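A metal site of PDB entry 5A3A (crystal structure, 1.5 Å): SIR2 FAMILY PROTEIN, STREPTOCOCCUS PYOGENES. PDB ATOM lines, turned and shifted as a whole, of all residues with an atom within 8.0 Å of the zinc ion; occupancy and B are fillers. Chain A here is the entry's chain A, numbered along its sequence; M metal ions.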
ATOM      1  N   GLN A 154      -1.911 -25.286   6.757  1.00  0.00           N
ATOM      2  CA  GLN A 154      -1.558 -26.529   7.479  1.00  0.00           C
ATOM      3  C   GLN A 154      -0.463 -27.274   6.746  1.00  0.00           C
ATOM      4  O   GLN A 154      -0.310 -27.156   5.538  1.00  0.00           O
ATOM      5  CB  GLN A 154      -2.806 -27.430   7.646  1.00  0.00           C
ATOM      6  CG  GLN A 154      -3.329 -27.972   6.321  1.00  0.00           C
ATOM      7  CD  GLN A 154      -4.718 -28.668   6.391  1.00  0.00           C
ATOM      8  OE1 GLN A 154      -5.494 -28.473   7.321  1.00  0.00           O
ATOM      9  NE2 GLN A 154      -5.074 -29.389   5.299  1.00  0.00           N
ATOM     10  N   CYS A 155       0.324 -28.077   7.476  1.00  0.00           N
ATOM     11  CA  CYS A 155       1.228 -28.997   6.819  1.00  0.00           C
ATOM     12  C   CYS A 155       0.509 -29.884   5.812  1.00  0.00           C
ATOM     13  O   CYS A 155      -0.474 -30.495   6.161  1.00  0.00           O
ATOM     14  CB  CYS A 155       1.840 -29.884   7.864  1.00  0.00           C
ATOM     15  SG  CYS A 155       2.933 -31.181   7.109  1.00  0.00           S
ATOM     16  N   SER A 156       1.013 -30.004   4.568  1.00  0.00           N
ATOM     17  CA  SER A 156       0.344 -30.833   3.576  1.00  0.00           C
ATOM     18  C   SER A 156       0.376 -32.359   3.846  1.00  0.00           C
ATOM     19  O   SER A 156      -0.458 -33.090   3.314  1.00  0.00           O
ATOM     20  CB  SER A 156       0.904 -30.571   2.171  1.00  0.00           C
ATOM     21  OG  SER A 156       2.310 -30.841   2.161  1.00  0.00           O
ATOM     22  N   GLN A 157       1.290 -32.790   4.741  1.00  0.00           N
ATOM     23  CA  GLN A 157       1.304 -34.149   5.263  1.00  0.00           C
ATOM     24  C   GLN A 157       0.625 -34.274   6.617  1.00  0.00           C
ATOM     25  O   GLN A 157       0.649 -35.359   7.205  1.00  0.00           O
ATOM     26  CB  GLN A 157       2.751 -34.619   5.427  1.00  0.00           C
ATOM     27  CG  GLN A 157       3.517 -34.542   4.128  1.00  0.00           C
ATOM     28  CD  GLN A 157       3.259 -35.744   3.309  1.00  0.00           C
ATOM     29  OE1 GLN A 157       3.734 -36.827   3.637  1.00  0.00           O
ATOM     30  NE2 GLN A 157       2.517 -35.570   2.211  1.00  0.00           N
ATOM     31  N   HIS A 158       0.028 -33.182   7.106  1.00  0.00           N
ATOM     32  CA  HIS A 158      -0.752 -33.172   8.369  1.00  0.00           C
ATOM     33  C   HIS A 158       0.122 -33.702   9.510  1.00  0.00           C
ATOM     34  O   HIS A 158      -0.375 -34.427  10.403  1.00  0.00           O
ATOM     35  CB  HIS A 158      -2.018 -34.029   8.286  1.00  0.00           C
ATOM     36  CG  HIS A 158      -3.094 -33.535   7.378  1.00  0.00           C
ATOM     37  ND1 HIS A 158      -2.869 -33.112   6.090  1.00  0.00           N
ATOM     38  CD2 HIS A 158      -4.441 -33.553   7.533  1.00  0.00           C
ATOM     39  CE1 HIS A 158      -4.029 -32.813   5.514  1.00  0.00           C
ATOM     40  NE2 HIS A 158      -4.982 -33.075   6.367  1.00  0.00           N
ATOM     41  N   CYS A 159       1.390 -33.337   9.545  1.00  0.00           N
ATOM     42  CA  CYS A 159       2.337 -34.049  10.432  1.00  0.00           C
ATOM     43  C   CYS A 159       2.185 -33.662  11.889  1.00  0.00           C
ATOM     44  O   CYS A 159       2.617 -34.401  12.794  1.00  0.00           O
ATOM     45  CB  CYS A 159       3.794 -33.836   9.973  1.00  0.00           C
ATOM     46  SG  CYS A 159       4.559 -32.375  10.492  1.00  0.00           S
ATOM     47  N   HIS A 160       1.595 -32.501  12.131  1.00  0.00           N
ATOM     48  CA  HIS A 160       1.281 -32.066  13.482  1.00  0.00           C
ATOM     49  C   HIS A 160       0.055 -31.147  13.453  1.00  0.00           C
ATOM     50  O   HIS A 160      -0.284 -30.583  12.395  1.00  0.00           O
ATOM     51  CB  HIS A 160       2.505 -31.387  14.133  1.00  0.00           C
ATOM     52  CG  HIS A 160       2.867 -30.069  13.534  1.00  0.00           C
ATOM     53  ND1 HIS A 160       3.244 -29.918  12.216  1.00  0.00           N
ATOM     54  CD2 HIS A 160       2.936 -28.841  14.081  1.00  0.00           C
ATOM     55  CE1 HIS A 160       3.552 -28.649  11.992  1.00  0.00           C
ATOM     56  NE2 HIS A 160       3.340 -27.977  13.095  1.00  0.00           N
ATOM     57  N   TYR A 164      -0.982 -22.195  10.736  1.00  0.00           N
ATOM     58  CA  TYR A 164      -0.040 -21.113  10.587  1.00  0.00           C
ATOM     59  C   TYR A 164      -0.657 -20.054   9.671  1.00  0.00           C
ATOM     60  O   TYR A 164      -1.679 -20.316   9.025  1.00  0.00           O
ATOM     61  CB  TYR A 164       1.249 -21.618   9.961  1.00  0.00           C
ATOM     62  CG  TYR A 164       1.980 -22.670  10.816  1.00  0.00           C
ATOM     63  CD1 TYR A 164       1.587 -23.961  10.807  1.00  0.00           C
ATOM     64  CD2 TYR A 164       3.062 -22.305  11.650  1.00  0.00           C
ATOM     65  CE1 TYR A 164       2.218 -24.918  11.582  1.00  0.00           C
ATOM     66  CE2 TYR A 164       3.715 -23.267  12.415  1.00  0.00           C
ATOM     67  CZ  TYR A 164       3.296 -24.563  12.371  1.00  0.00           C
ATOM     68  OH  TYR A 164       3.907 -25.532  13.116  1.00  0.00           O
ATOM     69  N   HIS A 189       7.294 -23.919   3.679  1.00  0.00           N
ATOM     70  CA  HIS A 189       7.387 -25.312   4.151  1.00  0.00           C
ATOM     71  C   HIS A 189       7.195 -25.477   5.665  1.00  0.00           C
ATOM     72  O   HIS A 189       7.538 -24.612   6.471  1.00  0.00           O
ATOM     73  CB  HIS A 189       8.747 -25.925   3.737  1.00  0.00           C
ATOM     74  CG  HIS A 189       8.920 -26.017   2.262  1.00  0.00           C
ATOM     75  ND1 HIS A 189       9.390 -24.969   1.513  1.00  0.00           N
ATOM     76  CD2 HIS A 189       8.652 -27.018   1.387  1.00  0.00           C
ATOM     77  CE1 HIS A 189       9.461 -25.338   0.240  1.00  0.00           C
ATOM     78  NE2 HIS A 189       8.972 -26.553   0.140  1.00  0.00           N
ATOM     79  N   CYS A 190       6.620 -26.599   6.029  1.00  0.00           N
ATOM     80  CA  CYS A 190       6.386 -26.977   7.398  1.00  0.00           C
ATOM     81  C   CYS A 190       7.697 -27.036   8.148  1.00  0.00           C
ATOM     82  O   CYS A 190       8.598 -27.691   7.672  1.00  0.00           O
ATOM     83  CB  CYS A 190       5.803 -28.365   7.424  1.00  0.00           C
ATOM     84  SG  CYS A 190       5.498 -29.087   9.068  1.00  0.00           S
ATOM     85  N   PRO A 191       7.785 -26.418   9.333  1.00  0.00           N
ATOM     86  CA  PRO A 191       9.018 -26.482  10.142  1.00  0.00           C
ATOM     87  C   PRO A 191       9.333 -27.871  10.700  1.00  0.00           C
ATOM     88  O   PRO A 191      10.519 -28.175  10.961  1.00  0.00           O
ATOM     89  CB  PRO A 191       8.762 -25.491  11.271  1.00  0.00           C
ATOM     90  CG  PRO A 191       7.289 -25.248  11.266  1.00  0.00           C
ATOM     91  CD  PRO A 191       6.876 -25.382   9.849  1.00  0.00           C
ATOM     92  N   GLU A 192       8.317 -28.707  10.860  1.00  0.00           N
ATOM     93  CA  GLU A 192       8.501 -30.019  11.459  1.00  0.00           C
ATOM     94  C   GLU A 192       8.959 -31.097  10.481  1.00  0.00           C
ATOM     95  O   GLU A 192       9.716 -32.004  10.878  1.00  0.00           O
ATOM     96  CB  GLU A 192       7.208 -30.455  12.176  1.00  0.00           C
ATOM     97  CG  GLU A 192       6.822 -29.526  13.296  1.00  0.00           C
ATOM     98  CD  GLU A 192       7.748 -29.650  14.479  1.00  0.00           C
ATOM     99  OE1 GLU A 192       7.822 -30.755  15.045  1.00  0.00           O
ATOM    100  OE2 GLU A 192       8.411 -28.655  14.810  1.00  0.00           O
ATOM    101  N   CYS A 193       8.507 -31.081   9.226  1.00  0.00           N
ATOM    102  CA  CYS A 193       8.811 -32.169   8.326  1.00  0.00           C
ATOM    103  C   CYS A 193       9.286 -31.729   6.939  1.00  0.00           C
ATOM    104  O   CYS A 193       9.578 -32.592   6.109  1.00  0.00           O
ATOM    105  CB  CYS A 193       7.641 -33.125   8.156  1.00  0.00           C
ATOM    106  SG  CYS A 193       6.304 -32.387   7.118  1.00  0.00           S
ATOM    107  N   GLU A 194       9.271 -30.412   6.706  1.00  0.00           N
ATOM    108  CA  GLU A 194       9.694 -29.763   5.469  1.00  0.00           C
ATOM    109  C   GLU A 194       8.780 -29.990   4.259  1.00  0.00           C
ATOM    110  O   GLU A 194       9.106 -29.584   3.143  1.00  0.00           O
ATOM    111  CB  GLU A 194      11.149 -30.101   5.120  1.00  0.00           C
ATOM    112  CG  GLU A 194      12.160 -29.348   5.975  1.00  0.00           C
ATOM    113  CD  GLU A 194      13.580 -29.453   5.448  1.00  0.00           C
ATOM    114  OE1 GLU A 194      13.892 -30.468   4.776  1.00  0.00           O
ATOM    115  OE2 GLU A 194      14.370 -28.524   5.715  1.00  0.00           O
ATOM    116  N   ALA A 195       7.604 -30.592   4.470  1.00  0.00           N
ATOM    117  CA  ALA A 195       6.608 -30.689   3.387  1.00  0.00           C
ATOM    118  C   ALA A 195       6.067 -29.281   3.095  1.00  0.00           C
ATOM    119  O   ALA A 195       6.094 -28.423   3.952  1.00  0.00           O
ATOM    120  CB  ALA A 195       5.470 -31.647   3.723  1.00  0.00           C
ATOM    121  N   PRO A 196       5.681 -29.041   1.841  1.00  0.00           N
ATOM    122  CA  PRO A 196       5.025 -27.700   1.596  1.00  0.00           C
ATOM    123  C   PRO A 196       3.797 -27.509   2.522  1.00  0.00           C
ATOM    124  O   PRO A 196       3.077 -28.474   2.831  1.00  0.00           O
ATOM    125  CB  PRO A 196       4.597 -27.778   0.130  1.00  0.00           C
ATOM    126  CG  PRO A 196       5.403 -28.927  -0.444  1.00  0.00           C
ATOM    127  CD  PRO A 196       5.602 -29.899   0.667  1.00  0.00           C
ATOM    128  N   PHE A 197       3.589 -26.272   2.985  1.00  0.00           N
ATOM    129  CA  PHE A 197       2.293 -25.880   3.524  1.00  0.00           C
ATOM    130  C   PHE A 197       1.256 -25.893   2.396  1.00  0.00           C
ATOM    131  O   PHE A 197       1.575 -25.698   1.211  1.00  0.00           O
ATOM    132  CB  PHE A 197       2.378 -24.511   4.107  1.00  0.00           C
ATOM    133  CG  PHE A 197       2.925 -24.437   5.534  1.00  0.00           C
ATOM    134  CD1 PHE A 197       2.389 -25.231   6.555  1.00  0.00           C
ATOM    135  CD2 PHE A 197       3.966 -23.610   5.860  1.00  0.00           C
ATOM    136  CE1 PHE A 197       2.852 -25.133   7.857  1.00  0.00           C
ATOM    137  CE2 PHE A 197       4.410 -23.498   7.163  1.00  0.00           C
ATOM    138  CZ  PHE A 197       3.874 -24.272   8.152  1.00  0.00           C
HETATM  139 ZN    ZN M   1       4.861 -31.218   8.494  1.00  0.00          ZN
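The nearest printed residue that does not touch the zinc ion is His 160 (4.3 Å).
The zinc ion is bound by the side-chain sulfur (SG) of Cys 190, the side-chain sulfur (SG) of Cys 193, the side-chain sulfur (SG) of Cys 159 and the side-chain sulfur (SG) of Cys 155.
The zinc ion has four donor atoms within binding distance.
The side-chain sulfur (SG) of Cys 190 lies close to the backbone NH (N) of Glu 192 (3.4 Å).
The backbone carbonyl oxygen (O) of Ala 195 is in hydrogen-bond range of the backbone NH (N) of Cys 190, 2.8 Å away.
The side-chain sulfur of Cys 193 sits close to the backbone NH of Ala 195 (3.5 Å).
A ring nitrogen (ND1) of His 160 lies close to the side-chain sulfur (SG) of Cys 159 (3.3 Å).
SG of Cys 155 sits close to N of Gln 157 (3.3 Å).
SG of Cys 155 lies close to N of His 158 (3.5 Å).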
